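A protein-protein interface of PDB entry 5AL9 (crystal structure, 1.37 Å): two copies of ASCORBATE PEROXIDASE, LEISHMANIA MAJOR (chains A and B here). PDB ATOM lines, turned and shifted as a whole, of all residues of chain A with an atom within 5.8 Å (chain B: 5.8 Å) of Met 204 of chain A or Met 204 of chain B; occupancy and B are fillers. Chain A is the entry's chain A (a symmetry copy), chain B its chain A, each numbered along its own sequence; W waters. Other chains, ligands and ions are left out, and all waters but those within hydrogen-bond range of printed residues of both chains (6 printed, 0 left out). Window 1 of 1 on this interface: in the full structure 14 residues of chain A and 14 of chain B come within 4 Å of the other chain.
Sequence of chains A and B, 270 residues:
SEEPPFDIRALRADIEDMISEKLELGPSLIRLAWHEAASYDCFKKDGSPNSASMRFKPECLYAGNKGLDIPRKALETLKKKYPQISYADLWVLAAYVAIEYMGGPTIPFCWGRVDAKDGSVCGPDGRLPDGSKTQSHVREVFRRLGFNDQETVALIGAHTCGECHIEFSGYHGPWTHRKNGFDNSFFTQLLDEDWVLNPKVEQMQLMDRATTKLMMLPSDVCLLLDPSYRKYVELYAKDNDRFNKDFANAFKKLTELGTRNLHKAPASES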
ATOM      1  N   SER A 132      13.511  -5.583  -0.637  1.00  0.00           N
ATOM      2  CA  SER A 132      13.433  -6.064  -2.007  1.00  0.00           C
ATOM      3  C   SER A 132      14.337  -7.272  -2.213  1.00  0.00           C
ATOM      4  O   SER A 132      14.340  -7.878  -3.285  1.00  0.00           O
ATOM      5  CB  SER A 132      13.832  -4.952  -2.971  1.00  0.00           C
ATOM      6  OG  SER A 132      15.220  -4.691  -2.884  1.00  0.00           O
ATOM      7  N   THR A 134      16.256 -11.054  -0.757  1.00  0.00           N
ATOM      8  CA  THR A 134      15.751 -12.317  -0.230  1.00  0.00           C
ATOM      9  C   THR A 134      16.712 -12.979   0.759  1.00  0.00           C
ATOM     10  O   THR A 134      17.442 -12.286   1.453  1.00  0.00           O
ATOM     11  CB  THR A 134      15.320 -13.269  -1.351  1.00  0.00           C
ATOM     12  OG1 THR A 134      16.390 -13.417  -2.289  1.00  0.00           O
ATOM     13  CG2 THR A 134      14.094 -12.704  -2.076  1.00  0.00           C
ATOM     14  N   GLN A 135      16.717 -14.307   0.829  1.00  0.00           N
ATOM     15  CA  GLN A 135      17.281 -14.960   2.023  1.00  0.00           C
ATOM     16  C   GLN A 135      18.794 -14.859   2.190  1.00  0.00           C
ATOM     17  O   GLN A 135      19.276 -14.855   3.320  1.00  0.00           O
ATOM     18  CB  GLN A 135      16.829 -16.421   2.135  1.00  0.00           C
ATOM     19  CG  GLN A 135      17.276 -17.325   1.011  1.00  0.00           C
ATOM     20  CD  GLN A 135      16.225 -17.448  -0.075  1.00  0.00           C
ATOM     21  OE1 GLN A 135      15.594 -16.463  -0.458  1.00  0.00           O
ATOM     22  NE2 GLN A 135      16.014 -18.664  -0.557  1.00  0.00           N
ATOM     23  N   TYR A 171       6.758   0.925  -0.305  1.00  0.00           N
ATOM     24  CA  TYR A 171       5.795  -0.168  -0.256  1.00  0.00           C
ATOM     25  C   TYR A 171       4.511   0.364   0.343  1.00  0.00           C
ATOM     26  O   TYR A 171       4.499   1.434   0.953  1.00  0.00           O
ATOM     27  CB  TYR A 171       6.325  -1.307   0.598  1.00  0.00           C
ATOM     28  CG  TYR A 171       7.534  -1.984   0.011  1.00  0.00           C
ATOM     29  CD1 TYR A 171       7.423  -2.775  -1.119  1.00  0.00           C
ATOM     30  CD2 TYR A 171       8.783  -1.844   0.607  1.00  0.00           C
ATOM     31  CE1 TYR A 171       8.531  -3.414  -1.655  1.00  0.00           C
ATOM     32  CE2 TYR A 171       9.893  -2.477   0.085  1.00  0.00           C
ATOM     33  CZ  TYR A 171       9.759  -3.259  -1.041  1.00  0.00           C
ATOM     34  OH  TYR A 171      10.850  -3.892  -1.571  1.00  0.00           O
ATOM     35  N   LEU A 197       1.560 -11.435  -7.472  1.00  0.00           N
ATOM     36  CA  LEU A 197       2.055 -10.103  -7.761  1.00  0.00           C
ATOM     37  C   LEU A 197       0.948  -9.064  -7.602  1.00  0.00           C
ATOM     38  O   LEU A 197      -0.166  -9.251  -8.079  1.00  0.00           O
ATOM     39  CB  LEU A 197       2.595 -10.067  -9.183  1.00  0.00           C
ATOM     40  CG  LEU A 197       3.163  -8.737  -9.669  1.00  0.00           C
ATOM     41  CD1 LEU A 197       4.406  -8.397  -8.871  1.00  0.00           C
ATOM     42  CD2 LEU A 197       3.460  -8.812 -11.161  1.00  0.00           C
ATOM     43  N   VAL A 201       1.190  -1.588  -7.236  1.00  0.00           N
ATOM     44  CA  VAL A 201       2.241  -0.922  -6.475  1.00  0.00           C
ATOM     45  C   VAL A 201       3.547  -1.020  -7.247  1.00  0.00           C
ATOM     46  O   VAL A 201       3.992  -2.116  -7.589  1.00  0.00           O
ATOM     47  CB  VAL A 201       2.406  -1.521  -5.058  1.00  0.00           C
ATOM     48  CG1 VAL A 201       3.513  -0.804  -4.304  1.00  0.00           C
ATOM     49  CG2 VAL A 201       1.102  -1.408  -4.297  1.00  0.00           C
ATOM     50  N   GLU A 202       4.157   0.126  -7.528  1.00  0.00           N
ATOM     51  CA  GLU A 202       5.333   0.160  -8.395  1.00  0.00           C
ATOM     52  C   GLU A 202       6.530  -0.575  -7.819  1.00  0.00           C
ATOM     53  O   GLU A 202       7.334  -1.143  -8.560  1.00  0.00           O
ATOM     54  CB  GLU A 202       5.706   1.597  -8.760  1.00  0.00           C
ATOM     55  CG  GLU A 202       4.858   2.142  -9.889  1.00  0.00           C
ATOM     56  CD  GLU A 202       5.184   3.580 -10.243  1.00  0.00           C
ATOM     57  OE1 GLU A 202       6.375   3.956 -10.203  1.00  0.00           O
ATOM     58  OE2 GLU A 202       4.241   4.327 -10.578  1.00  0.00           O
ATOM     59  N   GLN A 203       6.648  -0.571  -6.498  1.00  0.00           N
ATOM     60  CA  GLN A 203       7.665  -1.377  -5.851  1.00  0.00           C
ATOM     61  C   GLN A 203       7.099  -2.764  -5.647  1.00  0.00           C
ATOM     62  O   GLN A 203       6.073  -2.933  -4.984  1.00  0.00           O
ATOM     63  CB  GLN A 203       8.089  -0.773  -4.520  1.00  0.00           C
ATOM     64  CG  GLN A 203       8.806   0.546  -4.668  1.00  0.00           C
ATOM     65  CD  GLN A 203       9.715   0.847  -3.496  1.00  0.00           C
ATOM     66  OE1 GLN A 203      10.534   1.763  -3.559  1.00  0.00           O
ATOM     67  NE2 GLN A 203       9.579   0.076  -2.416  1.00  0.00           N
ATOM     68  N   MET A 204       7.781  -3.753  -6.210  1.00  0.00           N
ATOM     69  CA  MET A 204       7.275  -5.117  -6.205  1.00  0.00           C
ATOM     70  C   MET A 204       6.962  -5.640  -4.812  1.00  0.00           C
ATOM     71  O   MET A 204       7.836  -5.764  -3.946  1.00  0.00           O
ATOM     72  CB  MET A 204       8.247  -6.061  -6.895  1.00  0.00           C
ATOM     73  CG  MET A 204       7.668  -7.437  -7.134  1.00  0.00           C
ATOM     74  SD  MET A 204       8.941  -8.506  -7.812  1.00  0.00           S
ATOM     75  CE  MET A 204      10.044  -8.616  -6.408  1.00  0.00           C
ATOM     76  N   GLN A 205       5.686  -5.943  -4.613  1.00  0.00           N
ATOM     77  CA  GLN A 205       5.239  -6.610  -3.407  1.00  0.00           C
ATOM     78  C   GLN A 205       4.141  -7.591  -3.803  1.00  0.00           C
ATOM     79  O   GLN A 205       3.569  -7.490  -4.889  1.00  0.00           O
ATOM     80  CB  GLN A 205       4.745  -5.597  -2.380  1.00  0.00           C
ATOM     81  CG  GLN A 205       3.700  -4.638  -2.905  1.00  0.00           C
ATOM     82  CD  GLN A 205       3.272  -3.629  -1.859  1.00  0.00           C
ATOM     83  OE1 GLN A 205       4.039  -2.734  -1.487  1.00  0.00           O
ATOM     84  NE2 GLN A 205       2.046  -3.767  -1.373  1.00  0.00           N
ATOM     85  N   LEU A 206       3.879  -8.562  -2.942  1.00  0.00           N
ATOM     86  CA  LEU A 206       2.867  -9.556  -3.232  1.00  0.00           C
ATOM     87  C   LEU A 206       1.618  -9.230  -2.433  1.00  0.00           C
ATOM     88  O   LEU A 206       1.672  -8.500  -1.445  1.00  0.00           O
ATOM     89  CB  LEU A 206       3.382 -10.946  -2.857  1.00  0.00           C
ATOM     90  CG  LEU A 206       4.682 -11.315  -3.567  1.00  0.00           C
ATOM     91  CD1 LEU A 206       5.138 -12.707  -3.180  1.00  0.00           C
ATOM     92  CD2 LEU A 206       4.490 -11.218  -5.072  1.00  0.00           C
ATOM     93  N   MET A 216       2.974  -8.969   1.309  1.00  0.00           N
ATOM     94  CA  MET A 216       4.257  -9.504   1.738  1.00  0.00           C
ATOM     95  C   MET A 216       5.337  -8.910   0.860  1.00  0.00           C
ATOM     96  O   MET A 216       5.123  -8.700  -0.328  1.00  0.00           O
ATOM     97  CB  MET A 216       4.289 -11.029   1.626  1.00  0.00           C
ATOM     98  CG  MET A 216       3.406 -11.750   2.627  1.00  0.00           C
ATOM     99  SD  MET A 216       3.905 -11.540   4.352  1.00  0.00           S
ATOM    100  CE  MET A 216       3.253 -13.034   5.085  1.00  0.00           C
ATOM    101  N   LEU A 217       6.482  -8.625   1.460  1.00  0.00           N
ATOM    102  CA  LEU A 217       7.654  -8.170   0.723  1.00  0.00           C
ATOM    103  C   LEU A 217       8.434  -9.384   0.232  1.00  0.00           C
ATOM    104  O   LEU A 217       8.249 -10.484   0.742  1.00  0.00           O
ATOM    105  CB  LEU A 217       8.568  -7.388   1.663  1.00  0.00           C
ATOM    106  CG  LEU A 217       8.022  -6.213   2.474  1.00  0.00           C
ATOM    107  CD1 LEU A 217       9.000  -5.853   3.588  1.00  0.00           C
ATOM    108  CD2 LEU A 217       7.777  -5.029   1.577  1.00  0.00           C
ATOM    109  N   PRO A 218       9.331  -9.197  -0.748  1.00  0.00           N
ATOM    110  CA  PRO A 218      10.265 -10.271  -1.107  1.00  0.00           C
ATOM    111  C   PRO A 218      11.029 -10.805   0.113  1.00  0.00           C
ATOM    112  O   PRO A 218      11.248 -12.015   0.227  1.00  0.00           O
ATOM    113  CB  PRO A 218      11.217  -9.568  -2.076  1.00  0.00           C
ATOM    114  CG  PRO A 218      10.324  -8.568  -2.760  1.00  0.00           C
ATOM    115  CD  PRO A 218       9.453  -8.043  -1.658  1.00  0.00           C
ATOM    116  N   VAL A 221       8.665 -13.238   2.025  1.00  0.00           N
ATOM    117  CA  VAL A 221       8.389 -14.532   1.418  1.00  0.00           C
ATOM    118  C   VAL A 221       9.634 -15.386   1.288  1.00  0.00           C
ATOM    119  O   VAL A 221       9.535 -16.595   1.095  1.00  0.00           O
ATOM    120  CB  VAL A 221       7.650 -14.438   0.075  1.00  0.00           C
ATOM    121  CG1 VAL A 221       6.293 -13.753   0.262  1.00  0.00           C
ATOM    122  CG2 VAL A 221       8.504 -13.736  -0.971  1.00  0.00           C
ATOM    123  N   LEU A 225      10.753 -19.590   1.152  1.00  0.00           N
ATOM    124  CA  LEU A 225      11.592 -20.183   0.112  1.00  0.00           C
ATOM    125  C   LEU A 225      12.816 -20.904   0.662  1.00  0.00           C
ATOM    126  O   LEU A 225      13.288 -21.887   0.094  1.00  0.00           O
ATOM    127  CB  LEU A 225      12.046 -19.104  -0.873  1.00  0.00           C
ATOM    128  CG  LEU A 225      10.919 -18.353  -1.577  1.00  0.00           C
ATOM    129  CD1 LEU A 225      11.499 -17.357  -2.562  1.00  0.00           C
ATOM    130  CD2 LEU A 225      10.013 -19.348  -2.278  1.00  0.00           C
ATOM    131  N   SER B 132      17.042 -10.400  -9.946  1.00  0.00           N
ATOM    132  CA  SER B 132      16.336 -10.295  -8.679  1.00  0.00           C
ATOM    133  C   SER B 132      15.911  -8.858  -8.410  1.00  0.00           C
ATOM    134  O   SER B 132      15.221  -8.580  -7.428  1.00  0.00           O
ATOM    135  CB  SER B 132      17.229 -10.788  -7.545  1.00  0.00           C
ATOM    136  OG  SER B 132      18.287  -9.876  -7.311  1.00  0.00           O
ATOM    137  N   THR B 134      14.469  -4.847  -9.803  1.00  0.00           N
ATOM    138  CA  THR B 134      13.304  -4.384 -10.550  1.00  0.00           C
ATOM    139  C   THR B 134      13.584  -3.128 -11.376  1.00  0.00           C
ATOM    140  O   THR B 134      14.703  -2.934 -11.827  1.00  0.00           O
ATOM    141  CB  THR B 134      12.076  -4.228  -9.647  1.00  0.00           C
ATOM    142  OG1 THR B 134      12.411  -3.407  -8.524  1.00  0.00           O
ATOM    143  CG2 THR B 134      11.617  -5.600  -9.142  1.00  0.00           C
ATOM    144  N   GLN B 135      12.581  -2.278 -11.577  1.00  0.00           N
ATOM    145  CA  GLN B 135      12.671  -1.311 -12.685  1.00  0.00           C
ATOM    146  C   GLN B 135      13.697  -0.195 -12.519  1.00  0.00           C
ATOM    147  O   GLN B 135      14.229   0.287 -13.515  1.00  0.00           O
ATOM    148  CB  GLN B 135      11.298  -0.725 -13.037  1.00  0.00           C
ATOM    149  CG  GLN B 135      10.636   0.076 -11.941  1.00  0.00           C
ATOM    150  CD  GLN B 135       9.679  -0.763 -11.118  1.00  0.00           C
ATOM    151  OE1 GLN B 135       9.974  -1.910 -10.780  1.00  0.00           O
ATOM    152  NE2 GLN B 135       8.515  -0.207 -10.817  1.00  0.00           N
ATOM    153  N   TYR B 171      18.037 -19.668 -11.034  1.00  0.00           N
ATOM    154  CA  TYR B 171      16.625 -19.713 -11.394  1.00  0.00           C
ATOM    155  C   TYR B 171      16.385 -20.976 -12.193  1.00  0.00           C
ATOM    156  O   TYR B 171      17.329 -21.599 -12.682  1.00  0.00           O
ATOM    157  CB  TYR B 171      16.250 -18.500 -12.229  1.00  0.00           C
ATOM    158  CG  TYR B 171      16.336 -17.203 -11.471  1.00  0.00           C
ATOM    159  CD1 TYR B 171      15.422 -16.902 -10.475  1.00  0.00           C
ATOM    160  CD2 TYR B 171      17.323 -16.270 -11.773  1.00  0.00           C
ATOM    161  CE1 TYR B 171      15.487 -15.701  -9.785  1.00  0.00           C
ATOM    162  CE2 TYR B 171      17.397 -15.070 -11.096  1.00  0.00           C
ATOM    163  CZ  TYR B 171      16.478 -14.793 -10.108  1.00  0.00           C
ATOM    164  OH  TYR B 171      16.538 -13.608  -9.427  1.00  0.00           O
ATOM    165  N   LEU B 197       3.887 -16.582  -6.407  1.00  0.00           N
ATOM    166  CA  LEU B 197       5.149 -17.071  -5.888  1.00  0.00           C
ATOM    167  C   LEU B 197       5.312 -18.563  -6.170  1.00  0.00           C
ATOM    168  O   LEU B 197       4.395 -19.349  -5.960  1.00  0.00           O
ATOM    169  CB  LEU B 197       5.203 -16.822  -4.387  1.00  0.00           C
ATOM    170  CG  LEU B 197       6.466 -17.275  -3.661  1.00  0.00           C
ATOM    171  CD1 LEU B 197       7.646 -16.453  -4.141  1.00  0.00           C
ATOM    172  CD2 LEU B 197       6.274 -17.149  -2.156  1.00  0.00           C
ATOM    173  N   VAL B 201      11.283 -23.061  -5.721  1.00  0.00           N
ATOM    174  CA  VAL B 201      12.589 -22.597  -6.172  1.00  0.00           C
ATOM    175  C   VAL B 201      13.140 -21.608  -5.156  1.00  0.00           C
ATOM    176  O   VAL B 201      12.495 -20.609  -4.840  1.00  0.00           O
ATOM    177  CB  VAL B 201      12.528 -21.949  -7.576  1.00  0.00           C
ATOM    178  CG1 VAL B 201      13.906 -21.475  -8.003  1.00  0.00           C
ATOM    179  CG2 VAL B 201      11.987 -22.946  -8.579  1.00  0.00           C
ATOM    180  N   GLU B 202      14.330 -21.892  -4.639  1.00  0.00           N
ATOM    181  CA  GLU B 202      14.884 -21.097  -3.544  1.00  0.00           C
ATOM    182  C   GLU B 202      15.164 -19.655  -3.927  1.00  0.00           C
ATOM    183  O   GLU B 202      15.056 -18.752  -3.094  1.00  0.00           O
ATOM    184  CB  GLU B 202      16.138 -21.754  -2.966  1.00  0.00           C
ATOM    185  CG  GLU B 202      15.807 -22.865  -1.992  1.00  0.00           C
ATOM    186  CD  GLU B 202      17.034 -23.558  -1.434  1.00  0.00           C
ATOM    187  OE1 GLU B 202      18.051 -22.876  -1.184  1.00  0.00           O
ATOM    188  OE2 GLU B 202      16.969 -24.789  -1.232  1.00  0.00           O
ATOM    189  N   GLN B 203      15.516 -19.433  -5.187  1.00  0.00           N
ATOM    190  CA  GLN B 203      15.647 -18.077  -5.682  1.00  0.00           C
ATOM    191  C   GLN B 203      14.282 -17.615  -6.140  1.00  0.00           C
ATOM    192  O   GLN B 203      13.672 -18.230  -7.018  1.00  0.00           O
ATOM    193  CB  GLN B 203      16.647 -17.998  -6.827  1.00  0.00           C
ATOM    194  CG  GLN B 203      18.063 -18.295  -6.398  1.00  0.00           C
ATOM    195  CD  GLN B 203      19.090 -17.667  -7.316  1.00  0.00           C
ATOM    196  OE1 GLN B 203      20.276 -17.623  -6.990  1.00  0.00           O
ATOM    197  NE2 GLN B 203      18.643 -17.177  -8.473  1.00  0.00           N
ATOM    198  N   MET B 204      13.814 -16.524  -5.549  1.00  0.00           N
ATOM    199  CA  MET B 204      12.461 -16.050  -5.798  1.00  0.00           C
ATOM    200  C   MET B 204      12.163 -15.820  -7.271  1.00  0.00           C
ATOM    201  O   MET B 204      12.779 -14.983  -7.942  1.00  0.00           O
ATOM    202  CB  MET B 204      12.178 -14.777  -5.017  1.00  0.00           C
ATOM    203  CG  MET B 204      10.719 -14.377  -5.046  1.00  0.00           C
ATOM    204  SD  MET B 204      10.524 -12.791  -4.227  1.00  0.00           S
ATOM    205  CE  MET B 204      11.401 -11.733  -5.371  1.00  0.00           C
ATOM    206  N   GLN B 205      11.202 -16.590  -7.764  1.00  0.00           N
ATOM    207  CA  GLN B 205      10.673 -16.390  -9.098  1.00  0.00           C
ATOM    208  C   GLN B 205       9.174 -16.655  -9.043  1.00  0.00           C
ATOM    209  O   GLN B 205       8.677 -17.268  -8.098  1.00  0.00           O
ATOM    210  CB  GLN B 205      11.371 -17.306 -10.099  1.00  0.00           C
ATOM    211  CG  GLN B 205      11.366 -18.767  -9.712  1.00  0.00           C
ATOM    212  CD  GLN B 205      12.104 -19.628 -10.717  1.00  0.00           C
ATOM    213  OE1 GLN B 205      13.333 -19.567 -10.826  1.00  0.00           O
ATOM    214  NE2 GLN B 205      11.360 -20.435 -11.461  1.00  0.00           N
ATOM    215  N   LEU B 206       8.450 -16.156 -10.034  1.00  0.00           N
ATOM    216  CA  LEU B 206       7.013 -16.336 -10.065  1.00  0.00           C
ATOM    217  C   LEU B 206       6.678 -17.421 -11.072  1.00  0.00           C
ATOM    218  O   LEU B 206       7.480 -17.741 -11.947  1.00  0.00           O
ATOM    219  CB  LEU B 206       6.335 -15.024 -10.462  1.00  0.00           C
ATOM    220  CG  LEU B 206       6.686 -13.863  -9.535  1.00  0.00           C
ATOM    221  CD1 LEU B 206       5.974 -12.594  -9.956  1.00  0.00           C
ATOM    222  CD2 LEU B 206       6.328 -14.224  -8.101  1.00  0.00           C
ATOM    223  N   MET B 216       8.485 -16.166 -14.398  1.00  0.00           N
ATOM    224  CA  MET B 216       8.940 -14.798 -14.600  1.00  0.00           C
ATOM    225  C   MET B 216       9.864 -14.431 -13.459  1.00  0.00           C
ATOM    226  O   MET B 216       9.646 -14.849 -12.327  1.00  0.00           O
ATOM    227  CB  MET B 216       7.763 -13.822 -14.638  1.00  0.00           C
ATOM    228  CG  MET B 216       6.886 -13.944 -15.870  1.00  0.00           C
ATOM    229  SD  MET B 216       7.712 -13.519 -17.421  1.00  0.00           S
ATOM    230  CE  MET B 216       6.324 -13.002 -18.422  1.00  0.00           C
ATOM    231  N   LEU B 217      10.900 -13.670 -13.772  1.00  0.00           N
ATOM    232  CA  LEU B 217      11.802 -13.131 -12.763  1.00  0.00           C
ATOM    233  C   LEU B 217      11.237 -11.814 -12.244  1.00  0.00           C
ATOM    234  O   LEU B 217      10.387 -11.211 -12.889  1.00  0.00           O
ATOM    235  CB  LEU B 217      13.154 -12.828 -13.405  1.00  0.00           C
ATOM    236  CG  LEU B 217      13.898 -13.908 -14.191  1.00  0.00           C
ATOM    237  CD1 LEU B 217      15.000 -13.271 -15.031  1.00  0.00           C
ATOM    238  CD2 LEU B 217      14.471 -14.934 -13.251  1.00  0.00           C
ATOM    239  N   PRO B 218      11.716 -11.342 -11.083  1.00  0.00           N
ATOM    240  CA  PRO B 218      11.379  -9.983 -10.645  1.00  0.00           C
ATOM    241  C   PRO B 218      11.687  -8.935 -11.725  1.00  0.00           C
ATOM    242  O   PRO B 218      10.913  -7.991 -11.912  1.00  0.00           O
ATOM    243  CB  PRO B 218      12.290  -9.792  -9.432  1.00  0.00           C
ATOM    244  CG  PRO B 218      12.376 -11.179  -8.854  1.00  0.00           C
ATOM    245  CD  PRO B 218      12.485 -12.069 -10.056  1.00  0.00           C
ATOM    246  N   VAL B 221       8.792  -9.022 -14.328  1.00  0.00           N
ATOM    247  CA  VAL B 221       7.502  -8.479 -13.926  1.00  0.00           C
ATOM    248  C   VAL B 221       7.571  -6.995 -13.624  1.00  0.00           C
ATOM    249  O   VAL B 221       6.540  -6.327 -13.578  1.00  0.00           O
ATOM    250  CB  VAL B 221       6.845  -9.242 -12.767  1.00  0.00           C
ATOM    251  CG1 VAL B 221       6.592 -10.698 -13.165  1.00  0.00           C
ATOM    252  CG2 VAL B 221       7.680  -9.134 -11.498  1.00  0.00           C
ATOM    253  N   LEU B 225       4.986  -3.494 -13.680  1.00  0.00           N
ATOM    254  CA  LEU B 225       4.818  -2.579 -12.552  1.00  0.00           C
ATOM    255  C   LEU B 225       5.118  -1.128 -12.902  1.00  0.00           C
ATOM    256  O   LEU B 225       4.528  -0.201 -12.349  1.00  0.00           O
ATOM    257  CB  LEU B 225       5.714  -3.011 -11.389  1.00  0.00           C
ATOM    258  CG  LEU B 225       5.462  -4.423 -10.867  1.00  0.00           C
ATOM    259  CD1 LEU B 225       6.371  -4.706  -9.686  1.00  0.00           C
ATOM    260  CD2 LEU B 225       4.002  -4.561 -10.476  1.00  0.00           C
HETATM  261  O   HOH W   1       9.741  -2.836  -8.017  1.00  0.00           O
HETATM  262  O   HOH W   2       2.508  -0.379 -10.467  1.00  0.00           O
HETATM  263  O   HOH W   3      12.328 -23.137  -2.179  1.00  0.00           O
HETATM  264  O   HOH W   4      15.323 -15.778  -3.287  1.00  0.00           O
HETATM  265  O   HOH W   5      17.732 -20.796   0.496  1.00  0.00           O
HETATM  266  O   HOH W   6       8.135   2.567 -11.694  1.00  0.00           O
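Leu 197 of chain A touches Val 221 of chain B. Leu 225 of chain B touches Glu 202 of chain A. Met 204 of chain A touches Met 204 of chain B (CE to CE, 3.6 Å). Met 204 of chain A touches Pro 218 of chain B (SD to CB, 3.9 Å). SD of Met 204 of chain A touches CG2 of Val 221 of chain B (3.9 Å). Met 204 of chain B touches Pro 218 of chain A. Val 221 of chain A touches Leu 197 of chain B (CB to CD2, 3.8 Å). CD2 of Leu 225 of chain A touches O of Val 201 of chain B, at 3.8 Å. Leu 225 of chain A touches Glu 202 of chain B. Met 204 of chain B touches Leu 225 of chain A.
Water W6 lies within hydrogen-bond range of OE1 of Glu 202 of chain A and NE2 of Gln 135 of chain B. Water W5 bridges the side-chain carboxylate (OE1) of Glu 202 of chain B (2.7 Å) and the side-chain amide nitrogen (NE2) of Gln 135 of chain A (2.9 Å). Water W3 bridges the backbone carbonyl oxygen (O) of Leu 225 of chain A (2.8 Å) and the backbone NH (N) of Glu 202 of chain B (3.4 Å). Water W2 bridges O of Leu 225 of chain B and N of Glu 202 of chain A. Water W1 lies within hydrogen-bond range of the side-chain hydroxyl (OG1) of Thr 134 of chain B (2.8 Å), the backbone NH (N) of Met 204 of chain A (2.8 Å), the side-chain amide oxygen (OE1) of Gln 135 of chain B (2.9 Å) and the backbone carbonyl oxygen (O) of Glu 202 of chain A (3.0 Å). Water W4 lies within hydrogen-bond range of the side-chain hydroxyl (OG1) of Thr 134 of chain A (2.8 Å), the backbone NH (N) of Met 204 of chain B (2.8 Å), the side-chain amide oxygen (OE1) of Gln 135 of chain A (2.9 Å) and the backbone carbonyl oxygen (O) of Glu 202 of chain B (3.0 Å).
Gln 135 of chain A touches Glu 202 of chain B, and with the chains exchanged Glu 202 of chain A touches Gln 135 of chain B. Leu 197 of chain A touches Val 221 of chain B, and with the chains exchanged Val 221 of chain A touches Leu 197 of chain B. Val 201 of chain A touches Leu 225 of chain B, and with the chains exchanged Leu 225 of chain A touches Val 201 of chain B. Met 204 of chain A touches Leu 225 of chain B, and with the chains exchanged Leu 225 of chain A touches Met 204 of chain B. Positions printed for both chains: 132, 134, 135, 171, 197, 201, 202, 203, 204, 205, 206, 216, 217, 218, 221 and 225. Of the 15 pairs that touch across the chains among the printed residues, 15 have their exchanged pair printed and touching as well.
The backbone carbonyl oxygen (O) of Glu 202 of chain B lies within hydrogen-bond range of the side-chain amide nitrogen (NE2) of Gln 135 of chain A, 2.7 Å away. The side-chain amide nitrogen (NE2) of Gln 135 of chain B lies within hydrogen-bond range of the backbone carbonyl oxygen (O) of Glu 202 of chain A (2.7 Å).
Printed residues of chain B within 4 Å of Gln 135 of chain A: Glu 202 (2.7 Å). Printed residues of chain B within 4 Å of Leu 197 of chain A: Val 221. Of the printed residues of chain B, Met 204 of chain A touches Met 204, Pro 218, Val 221 and Leu 225. Met 216 of chain A touches none of the printed residues of chain B. Of the printed residues of chain B, Pro 218 of chain A touches Met 204. Printed residues of chain A within 4 Å of Glu 202 of chain B: Gln 135 (2.7 Å) and Leu 225 (3.4 Å). Met 204 of chain B touches four residues of chain A.
Hydrophobic or aromatic side chains of chain A within 4 Å of the printed part of chain B: Leu 197, Met 204, Pro 218, Val 221 and Leu 225. Printed residues of chain B that touch a printed residue of chain A: Gln 135, Leu 197, Val 201, Glu 202, Met 204, Pro 218, Val 221 and Leu 225. Hydrophobic or aromatic side chains of chain B within 4 Å of the printed part of chain A: Leu 197, Met 204, Pro 218, Val 221 and Leu 225. Along chain B the printed residues that touch a printed residue of chain A span positions 135 to 225. Among the printed residues, 15 pairs touch across the chains. Among the printed residues, no Asp or Glu carboxylate lies within 4 Å of a Lys or Arg side-chain nitrogen of the other chain.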
